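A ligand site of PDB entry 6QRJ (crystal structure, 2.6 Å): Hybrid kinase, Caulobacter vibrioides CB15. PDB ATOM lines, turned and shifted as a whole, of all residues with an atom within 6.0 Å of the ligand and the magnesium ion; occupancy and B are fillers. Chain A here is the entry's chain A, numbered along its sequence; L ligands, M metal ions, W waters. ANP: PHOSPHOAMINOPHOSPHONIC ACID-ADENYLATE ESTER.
Merely in contact with the magnesium ion: Lys 130 (3.4 Å).
Of the 28 residues printed, 2 come within 4 Å of the magnesium ion.
The nearest printed residue that does not touch the magnesium ion is Asn 123 (4.9 Å).
The backbone NH (N) of Gly 187 lies within hydrogen-bond range of an oxygen (O1G) of the ligand (3.3 Å).
An oxygen (O2B) of the ligand lies within salt-bridge range of the side-chain amino group of Lys 130 (3.9 Å).
The backbone carbonyl oxygen of Gln 174 is in hydrogen-bond range of an oxygen (O2') of the ligand, at 3.3 Å.
N of Leu 190 sits at hydrogen-bond distance from O1A of the ligand.
The side-chain hydroxyl (OG1) of Thr 175 sits at hydrogen-bond distance from an oxygen (O2') of the ligand, at 2.5 Å.
The backbone NH of Leu 188 sits at hydrogen-bond distance from an oxygen (O1G) of the ligand.
The backbone NH (N) of Gly 189 sits at hydrogen-bond distance from an oxygen (O1G) of the ligand.
OD2 of Asp 155 sits at hydrogen-bond distance from N6 of the ligand (3.3 Å).
Residues that only touch the ligand: Phe 216 (3.5 Å), Phe 131 (3.6 Å), Val 173 (3.6 Å), Ile 168 (3.6 Å), Ala 186 (3.8 Å), Gly 185 (3.9 Å), Val 160 (3.9 Å), Asp 56 (3.9 Å), Ala 128 (3.97 Å) and Gly 159 (3.99 Å).
Hydrophobic or aromatic side chains that line the ligand: Phe 131, Val 160, Ile 168, Ala 186, Leu 190 and Phe 216.
Of the 28 residues printed, 19 come within 4 Å of the ligand.
Water W5 lies within hydrogen-bond range of N1 of the ligand (2.5 Å), OD1 of Asp 155 (2.6 Å) and N of Gly 159 (3.4 Å).
Water W1 lies within hydrogen-bond range of O of Phe 124 (2.7 Å), N6 of the ligand (2.7 Å), OD2 of Asp 155 (3.2 Å) and N of Ala 128 (3.3 Å).
Water W2 bridges the side-chain amide nitrogen of Asn 127 (2.8 Å) and a nitrogen (N7) of the ligand (3.0 Å).
The magnesium ion is bound by water W3 (1.7 Å), O1B of the ligand (2.0 Å), OD1 of Asn 127 (2.2 Å) and O3G of the ligand (2.4 Å).
The magnesium ion has four donor atoms within binding distance.
The backbone NH (N) of Asp 155 lies within hydrogen-bond range of the backbone carbonyl oxygen (O) of Ala 214 (3.0 Å).
The backbone carbonyl oxygen of Gly 189 is in hydrogen-bond range of the side-chain amide nitrogen of Asn 123, at 2.6 Å.
The side-chain amide nitrogen of Asn 127 sits close to the backbone carbonyl oxygen of Asn 123, at 3.2 Å.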
ATOM      1  N   ASP A  56     -22.404  -1.407   0.497  1.00  0.00           N
ATOM      2  CA  ASP A  56     -20.965  -1.563   0.203  1.00  0.00           C
ATOM      3  C   ASP A  56     -20.837  -1.414  -1.293  1.00  0.00           C
ATOM      4  O   ASP A  56     -20.060  -0.577  -1.768  1.00  0.00           O
ATOM      5  CB  ASP A  56     -20.387  -2.903   0.690  1.00  0.00           C
ATOM      6  CG  ASP A  56     -19.901  -2.936   2.142  1.00  0.00           C
ATOM      7  OD1 ASP A  56     -19.981  -1.866   2.826  1.00  0.00           O
ATOM      8  OD2 ASP A  56     -19.438  -4.052   2.604  1.00  0.00           O
ATOM      9  N   ASN A 123     -11.740   0.874   7.832  1.00  0.00           N
ATOM     10  CA  ASN A 123     -11.592  -0.285   6.934  1.00  0.00           C
ATOM     11  C   ASN A 123     -10.334  -1.024   7.379  1.00  0.00           C
ATOM     12  O   ASN A 123     -10.399  -2.217   7.554  1.00  0.00           O
ATOM     13  CB  ASN A 123     -11.716   0.089   5.455  1.00  0.00           C
ATOM     14  CG  ASN A 123     -13.155   0.384   5.072  1.00  0.00           C
ATOM     15  OD1 ASN A 123     -13.988   0.621   5.942  1.00  0.00           O
ATOM     16  ND2 ASN A 123     -13.439   0.395   3.791  1.00  0.00           N
ATOM     17  N   PHE A 124      -9.237  -0.334   7.581  1.00  0.00           N
ATOM     18  CA  PHE A 124      -7.949  -0.954   7.985  1.00  0.00           C
ATOM     19  C   PHE A 124      -8.064  -1.630   9.351  1.00  0.00           C
ATOM     20  O   PHE A 124      -7.454  -2.686   9.532  1.00  0.00           O
ATOM     21  CB  PHE A 124      -6.879   0.112   8.116  1.00  0.00           C
ATOM     22  CG  PHE A 124      -6.289   0.530   6.804  1.00  0.00           C
ATOM     23  CD1 PHE A 124      -6.280  -0.336   5.727  1.00  0.00           C
ATOM     24  CD2 PHE A 124      -5.662   1.754   6.675  1.00  0.00           C
ATOM     25  CE1 PHE A 124      -5.682   0.039   4.535  1.00  0.00           C
ATOM     26  CE2 PHE A 124      -5.110   2.133   5.468  1.00  0.00           C
ATOM     27  CZ  PHE A 124      -5.123   1.280   4.405  1.00  0.00           C
ATOM     28  N   GLY A 126     -11.001  -2.520  11.315  1.00  0.00           N
ATOM     29  CA  GLY A 126     -11.864  -3.712  11.204  1.00  0.00           C
ATOM     30  C   GLY A 126     -11.075  -4.880  10.669  1.00  0.00           C
ATOM     31  O   GLY A 126     -11.078  -5.929  11.300  1.00  0.00           O
ATOM     32  N   ASN A 127     -10.406  -4.714   9.537  1.00  0.00           N
ATOM     33  CA  ASN A 127      -9.658  -5.832   8.911  1.00  0.00           C
ATOM     34  C   ASN A 127      -8.737  -6.399   9.987  1.00  0.00           C
ATOM     35  O   ASN A 127      -8.765  -7.591  10.240  1.00  0.00           O
ATOM     36  CB  ASN A 127      -8.878  -5.376   7.664  1.00  0.00           C
ATOM     37  CG  ASN A 127      -9.747  -5.181   6.441  1.00  0.00           C
ATOM     38  OD1 ASN A 127     -10.834  -5.742   6.354  1.00  0.00           O
ATOM     39  ND2 ASN A 127      -9.258  -4.424   5.460  1.00  0.00           N
ATOM     40  N   ALA A 128      -7.980  -5.524  10.636  1.00  0.00           N
ATOM     41  CA  ALA A 128      -6.927  -5.879  11.604  1.00  0.00           C
ATOM     42  C   ALA A 128      -7.555  -6.672  12.739  1.00  0.00           C
ATOM     43  O   ALA A 128      -7.092  -7.742  13.018  1.00  0.00           O
ATOM     44  CB  ALA A 128      -6.257  -4.628  12.097  1.00  0.00           C
ATOM     45  N   LYS A 130     -10.360  -8.248  12.710  1.00  0.00           N
ATOM     46  CA  LYS A 130     -10.947  -9.499  12.182  1.00  0.00           C
ATOM     47  C   LYS A 130      -9.800 -10.505  12.034  1.00  0.00           C
ATOM     48  O   LYS A 130      -9.947 -11.607  12.507  1.00  0.00           O
ATOM     49  CB  LYS A 130     -11.676  -9.250  10.867  1.00  0.00           C
ATOM     50  CG  LYS A 130     -12.527 -10.420  10.375  1.00  0.00           C
ATOM     51  CD  LYS A 130     -12.571 -10.518   8.894  1.00  0.00           C
ATOM     52  CE  LYS A 130     -12.781  -9.164   8.233  1.00  0.00           C
ATOM     53  NZ  LYS A 130     -12.910  -9.317   6.765  1.00  0.00           N
ATOM     54  N   PHE A 131      -8.649 -10.092  11.509  1.00  0.00           N
ATOM     55  CA  PHE A 131      -7.596 -11.044  11.093  1.00  0.00           C
ATOM     56  C   PHE A 131      -6.596 -11.401  12.209  1.00  0.00           C
ATOM     57  O   PHE A 131      -5.821 -12.344  11.990  1.00  0.00           O
ATOM     58  CB  PHE A 131      -6.914 -10.508   9.841  1.00  0.00           C
ATOM     59  CG  PHE A 131      -7.784 -10.689   8.631  1.00  0.00           C
ATOM     60  CD1 PHE A 131      -8.164 -11.949   8.238  1.00  0.00           C
ATOM     61  CD2 PHE A 131      -8.312  -9.594   7.956  1.00  0.00           C
ATOM     62  CE1 PHE A 131      -9.011 -12.135   7.162  1.00  0.00           C
ATOM     63  CE2 PHE A 131      -9.169  -9.773   6.888  1.00  0.00           C
ATOM     64  CZ  PHE A 131      -9.516 -11.042   6.494  1.00  0.00           C
ATOM     65  N   ASP A 155      -0.785  -4.776  13.209  1.00  0.00           N
ATOM     66  CA  ASP A 155      -1.547  -5.878  13.814  1.00  0.00           C
ATOM     67  C   ASP A 155      -0.607  -7.064  13.945  1.00  0.00           C
ATOM     68  O   ASP A 155       0.162  -7.270  13.040  1.00  0.00           O
ATOM     69  CB  ASP A 155      -2.807  -6.138  13.004  1.00  0.00           C
ATOM     70  CG  ASP A 155      -2.635  -6.326  11.495  1.00  0.00           C
ATOM     71  OD1 ASP A 155      -2.234  -7.494  11.136  1.00  0.00           O
ATOM     72  OD2 ASP A 155      -2.917  -5.317  10.664  1.00  0.00           O
ATOM     73  N   GLY A 157      -1.275 -10.036  13.448  1.00  0.00           N
ATOM     74  CA  GLY A 157      -1.991 -11.097  12.710  1.00  0.00           C
ATOM     75  C   GLY A 157      -1.040 -12.029  11.976  1.00  0.00           C
ATOM     76  O   GLY A 157       0.118 -12.163  12.339  1.00  0.00           O
ATOM     77  N   PRO A 158      -1.519 -12.727  10.928  1.00  0.00           N
ATOM     78  CA  PRO A 158      -0.723 -13.707  10.185  1.00  0.00           C
ATOM     79  C   PRO A 158      -0.011 -13.075   8.984  1.00  0.00           C
ATOM     80  O   PRO A 158       0.653 -13.806   8.280  1.00  0.00           O
ATOM     81  CB  PRO A 158      -1.813 -14.647   9.695  1.00  0.00           C
ATOM     82  CG  PRO A 158      -2.906 -13.685   9.291  1.00  0.00           C
ATOM     83  CD  PRO A 158      -2.889 -12.628  10.379  1.00  0.00           C
ATOM     84  N   GLY A 159      -0.212 -11.778   8.766  1.00  0.00           N
ATOM     85  CA  GLY A 159       0.498 -10.947   7.781  1.00  0.00           C
ATOM     86  C   GLY A 159       0.032 -11.250   6.380  1.00  0.00           C
ATOM     87  O   GLY A 159      -0.835 -12.132   6.253  1.00  0.00           O
ATOM     88  N   VAL A 160       0.626 -10.590   5.377  1.00  0.00           N
ATOM     89  CA  VAL A 160       0.246 -10.699   3.930  1.00  0.00           C
ATOM     90  C   VAL A 160       1.467 -11.163   3.114  1.00  0.00           C
ATOM     91  O   VAL A 160       2.495 -10.465   3.181  1.00  0.00           O
ATOM     92  CB  VAL A 160      -0.262  -9.342   3.401  1.00  0.00           C
ATOM     93  CG1 VAL A 160      -0.604  -9.372   1.921  1.00  0.00           C
ATOM     94  CG2 VAL A 160      -1.464  -8.870   4.197  1.00  0.00           C
ATOM     95  N   ILE A 168      -4.823  -7.376  -3.224  1.00  0.00           N
ATOM     96  CA  ILE A 168      -5.911  -7.292  -2.209  1.00  0.00           C
ATOM     97  C   ILE A 168      -6.628  -5.917  -2.201  1.00  0.00           C
ATOM     98  O   ILE A 168      -7.700  -5.842  -1.547  1.00  0.00           O
ATOM     99  CB  ILE A 168      -5.382  -7.714  -0.807  1.00  0.00           C
ATOM    100  CG1 ILE A 168      -4.151  -6.924  -0.355  1.00  0.00           C
ATOM    101  CG2 ILE A 168      -5.128  -9.223  -0.764  1.00  0.00           C
ATOM    102  CD1 ILE A 168      -3.754  -7.140   1.114  1.00  0.00           C
ATOM    103  N   PHE A 169      -6.125  -4.870  -2.872  1.00  0.00           N
ATOM    104  CA  PHE A 169      -6.771  -3.520  -2.921  1.00  0.00           C
ATOM    105  C   PHE A 169      -7.761  -3.448  -4.105  1.00  0.00           C
ATOM    106  O   PHE A 169      -8.280  -2.345  -4.426  1.00  0.00           O
ATOM    107  CB  PHE A 169      -5.729  -2.396  -3.022  1.00  0.00           C
ATOM    108  CG  PHE A 169      -4.934  -2.138  -1.769  1.00  0.00           C
ATOM    109  CD1 PHE A 169      -5.282  -1.129  -0.903  1.00  0.00           C
ATOM    110  CD2 PHE A 169      -3.828  -2.911  -1.467  1.00  0.00           C
ATOM    111  CE1 PHE A 169      -4.559  -0.918   0.265  1.00  0.00           C
ATOM    112  CE2 PHE A 169      -3.080  -2.668  -0.320  1.00  0.00           C
ATOM    113  CZ  PHE A 169      -3.450  -1.678   0.546  1.00  0.00           C
ATOM    114  N   GLU A 170      -7.999  -4.575  -4.771  1.00  0.00           N
ATOM    115  CA  GLU A 170      -8.904  -4.663  -5.951  1.00  0.00           C
ATOM    116  C   GLU A 170     -10.272  -5.179  -5.472  1.00  0.00           C
ATOM    117  O   GLU A 170     -10.356  -5.732  -4.358  1.00  0.00           O
ATOM    118  CB  GLU A 170      -8.295  -5.558  -7.040  1.00  0.00           C
ATOM    119  CG  GLU A 170      -6.987  -5.020  -7.625  1.00  0.00           C
ATOM    120  CD  GLU A 170      -6.154  -6.039  -8.389  1.00  0.00           C
ATOM    121  OE1 GLU A 170      -4.945  -6.164  -8.061  1.00  0.00           O
ATOM    122  OE2 GLU A 170      -6.691  -6.686  -9.331  1.00  0.00           O
ATOM    123  N   VAL A 173     -11.662  -9.328  -4.382  1.00  0.00           N
ATOM    124  CA  VAL A 173     -10.478 -10.169  -4.046  1.00  0.00           C
ATOM    125  C   VAL A 173     -10.450 -10.409  -2.523  1.00  0.00           C
ATOM    126  O   VAL A 173     -10.544  -9.387  -1.768  1.00  0.00           O
ATOM    127  CB  VAL A 173      -9.172  -9.547  -4.587  1.00  0.00           C
ATOM    128  CG1 VAL A 173      -9.240  -9.280  -6.081  1.00  0.00           C
ATOM    129  CG2 VAL A 173      -8.804  -8.287  -3.819  1.00  0.00           C
ATOM    130  N   GLN A 174     -10.281 -11.688  -2.114  1.00  0.00           N
ATOM    131  CA  GLN A 174     -10.704 -12.309  -0.820  1.00  0.00           C
ATOM    132  C   GLN A 174      -9.513 -13.056  -0.156  1.00  0.00           C
ATOM    133  O   GLN A 174      -8.344 -12.662  -0.440  1.00  0.00           O
ATOM    134  CB  GLN A 174     -11.946 -13.171  -1.110  1.00  0.00           C
ATOM    135  CG  GLN A 174     -11.713 -14.503  -1.849  1.00  0.00           C
ATOM    136  CD  GLN A 174     -11.531 -14.516  -3.354  1.00  0.00           C
ATOM    137  OE1 GLN A 174     -11.507 -13.500  -4.049  1.00  0.00           O
ATOM    138  NE2 GLN A 174     -11.395 -15.717  -3.907  1.00  0.00           N
ATOM    139  N   THR A 175      -9.766 -14.034   0.751  1.00  0.00           N
ATOM    140  CA  THR A 175      -8.758 -14.978   1.367  1.00  0.00           C
ATOM    141  C   THR A 175      -9.154 -16.439   1.112  1.00  0.00           C
ATOM    142  O   THR A 175      -9.920 -16.979   1.954  1.00  0.00           O
ATOM    143  CB  THR A 175      -8.641 -14.895   2.911  1.00  0.00           C
ATOM    144  OG1 THR A 175      -8.597 -13.550   3.375  1.00  0.00           O
ATOM    145  CG2 THR A 175      -7.434 -15.624   3.455  1.00  0.00           C
ATOM    146  N   GLY A 185     -17.578 -10.094   3.122  1.00  0.00           N
ATOM    147  CA  GLY A 185     -18.275 -10.940   2.127  1.00  0.00           C
ATOM    148  C   GLY A 185     -18.066 -10.388   0.731  1.00  0.00           C
ATOM    149  O   GLY A 185     -17.635 -11.139  -0.187  1.00  0.00           O
ATOM    150  N   ALA A 186     -18.334  -9.096   0.563  1.00  0.00           N
ATOM    151  CA  ALA A 186     -18.157  -8.366  -0.710  1.00  0.00           C
ATOM    152  C   ALA A 186     -16.692  -8.488  -1.123  1.00  0.00           C
ATOM    153  O   ALA A 186     -16.443  -8.769  -2.308  1.00  0.00           O
ATOM    154  CB  ALA A 186     -18.534  -6.919  -0.480  1.00  0.00           C
ATOM    155  N   GLY A 187     -15.788  -8.290  -0.160  1.00  0.00           N
ATOM    156  CA  GLY A 187     -14.358  -8.086  -0.425  1.00  0.00           C
ATOM    157  C   GLY A 187     -14.158  -6.736  -1.085  1.00  0.00           C
ATOM    158  O   GLY A 187     -13.470  -6.661  -2.148  1.00  0.00           O
ATOM    159  N   LEU A 188     -14.764  -5.693  -0.510  1.00  0.00           N
ATOM    160  CA  LEU A 188     -14.719  -4.318  -1.063  1.00  0.00           C
ATOM    161  C   LEU A 188     -14.039  -3.328  -0.115  1.00  0.00           C
ATOM    162  O   LEU A 188     -13.657  -2.266  -0.567  1.00  0.00           O
ATOM    163  CB  LEU A 188     -16.144  -3.859  -1.387  1.00  0.00           C
ATOM    164  CG  LEU A 188     -16.513  -3.877  -2.874  1.00  0.00           C
ATOM    165  CD1 LEU A 188     -16.243  -5.229  -3.499  1.00  0.00           C
ATOM    166  CD2 LEU A 188     -17.974  -3.508  -3.065  1.00  0.00           C
ATOM    167  N   GLY A 189     -13.908  -3.632   1.153  1.00  0.00           N
ATOM    168  CA  GLY A 189     -13.415  -2.670   2.142  1.00  0.00           C
ATOM    169  C   GLY A 189     -12.104  -1.985   1.744  1.00  0.00           C
ATOM    170  O   GLY A 189     -12.016  -0.766   1.901  1.00  0.00           O
ATOM    171  N   LEU A 190     -11.138  -2.722   1.211  1.00  0.00           N
ATOM    172  CA  LEU A 190      -9.893  -2.102   0.712  1.00  0.00           C
ATOM    173  C   LEU A 190     -10.144  -1.436  -0.634  1.00  0.00           C
ATOM    174  O   LEU A 190      -9.611  -0.322  -0.809  1.00  0.00           O
ATOM    175  CB  LEU A 190      -8.752  -3.134   0.635  1.00  0.00           C
ATOM    176  CG  LEU A 190      -8.177  -3.516   1.995  1.00  0.00           C
ATOM    177  CD1 LEU A 190      -7.158  -4.625   1.845  1.00  0.00           C
ATOM    178  CD2 LEU A 190      -7.537  -2.334   2.706  1.00  0.00           C
ATOM    179  N   ALA A 191     -10.906  -2.031  -1.554  1.00  0.00           N
ATOM    180  CA  ALA A 191     -11.221  -1.358  -2.844  1.00  0.00           C
ATOM    181  C   ALA A 191     -11.728   0.071  -2.572  1.00  0.00           C
ATOM    182  O   ALA A 191     -11.282   1.011  -3.239  1.00  0.00           O
ATOM    183  CB  ALA A 191     -12.247  -2.119  -3.620  1.00  0.00           C
ATOM    184  N   ALA A 214       1.133  -7.342   9.959  1.00  0.00           N
ATOM    185  CA  ALA A 214       0.808  -6.526   8.785  1.00  0.00           C
ATOM    186  C   ALA A 214       0.700  -5.099   9.278  1.00  0.00           C
ATOM    187  O   ALA A 214       0.103  -4.915  10.339  1.00  0.00           O
ATOM    188  CB  ALA A 214      -0.517  -6.943   8.198  1.00  0.00           C
ATOM    189  N   PHE A 216      -0.818  -1.562   7.710  1.00  0.00           N
ATOM    190  CA  PHE A 216      -1.587  -0.936   6.615  1.00  0.00           C
ATOM    191  C   PHE A 216      -1.364   0.569   6.722  1.00  0.00           C
ATOM    192  O   PHE A 216      -1.403   1.135   7.829  1.00  0.00           O
ATOM    193  CB  PHE A 216      -3.034  -1.390   6.713  1.00  0.00           C
ATOM    194  CG  PHE A 216      -3.332  -2.634   5.917  1.00  0.00           C
ATOM    195  CD1 PHE A 216      -3.197  -3.887   6.489  1.00  0.00           C
ATOM    196  CD2 PHE A 216      -3.758  -2.548   4.587  1.00  0.00           C
ATOM    197  CE1 PHE A 216      -3.448  -5.039   5.744  1.00  0.00           C
ATOM    198  CE2 PHE A 216      -4.005  -3.688   3.836  1.00  0.00           C
ATOM    199  CZ  PHE A 216      -3.850  -4.934   4.429  1.00  0.00           C
HETATM  200  PG  ANP L   1     -15.094  -6.694   3.204  1.00  0.00           P
HETATM  201  O1G ANP L   1     -16.025  -6.004   2.251  1.00  0.00           O
HETATM  202  O2G ANP L   1     -15.725  -6.966   4.533  1.00  0.00           O
HETATM  203  O3G ANP L   1     -14.116  -5.702   3.822  1.00  0.00           O
HETATM  204  PB  ANP L   1     -12.823  -8.241   3.292  1.00  0.00           P
HETATM  205  O1B ANP L   1     -12.346  -7.483   4.603  1.00  0.00           O
HETATM  206  O2B ANP L   1     -12.290  -9.616   2.965  1.00  0.00           O
HETATM  207  N3B ANP L   1     -14.332  -8.013   2.787  1.00  0.00           N
HETATM  208  PA  ANP L   1     -11.038  -6.230   2.200  1.00  0.00           P
HETATM  209  O1A ANP L   1     -11.156  -5.578   0.875  1.00  0.00           O
HETATM  210  O2A ANP L   1     -11.191  -5.509   3.528  1.00  0.00           O
HETATM  211  O3A ANP L   1     -12.083  -7.480   2.079  1.00  0.00           O
HETATM  212  O5' ANP L   1      -9.700  -7.050   2.261  1.00  0.00           O
HETATM  213  C5' ANP L   1      -9.222  -7.759   1.133  1.00  0.00           C
HETATM  214  C4' ANP L   1      -8.359  -8.874   1.675  1.00  0.00           C
HETATM  215  O4' ANP L   1      -7.170  -8.381   2.347  1.00  0.00           O
HETATM  216  C3' ANP L   1      -9.033  -9.704   2.752  1.00  0.00           C
HETATM  217  O3' ANP L   1      -9.839 -10.607   2.017  1.00  0.00           O
HETATM  218  C2' ANP L   1      -7.815 -10.366   3.403  1.00  0.00           C
HETATM  219  O2' ANP L   1      -7.603 -11.436   2.514  1.00  0.00           O
HETATM  220  C1' ANP L   1      -6.728  -9.300   3.322  1.00  0.00           C
HETATM  221  N9  ANP L   1      -6.448  -8.519   4.498  1.00  0.00           N
HETATM  222  C8  ANP L   1      -6.894  -7.249   4.796  1.00  0.00           C
HETATM  223  N7  ANP L   1      -6.447  -6.810   5.959  1.00  0.00           N
HETATM  224  C5  ANP L   1      -5.630  -7.824   6.410  1.00  0.00           C
HETATM  225  C6  ANP L   1      -4.832  -7.947   7.550  1.00  0.00           C
HETATM  226  N6  ANP L   1      -4.735  -7.017   8.495  1.00  0.00           N
HETATM  227  N1  ANP L   1      -4.101  -9.084   7.660  1.00  0.00           N
HETATM  228  C2  ANP L   1      -4.188 -10.021   6.723  1.00  0.00           C
HETATM  229  N3  ANP L   1      -4.926 -10.014   5.609  1.00  0.00           N
HETATM  230  C4  ANP L   1      -5.615  -8.872   5.514  1.00  0.00           C
HETATM  231 MG    MG M   1     -12.961  -6.080   5.864  1.00  0.00          MG
HETATM  232  O   HOH W   1      -5.445  -4.416   8.901  1.00  0.00           O
HETATM  233  O   HOH W   2      -6.597  -3.794   5.767  1.00  0.00           O
HETATM  234  O   HOH W   3     -12.490  -4.584   5.116  1.00  0.00           O
HETATM  235  O   HOH W   4     -10.595  -6.081  -1.742  1.00  0.00           O
HETATM  236  O   HOH W   5      -2.633  -9.565   9.589  1.00  0.00           O
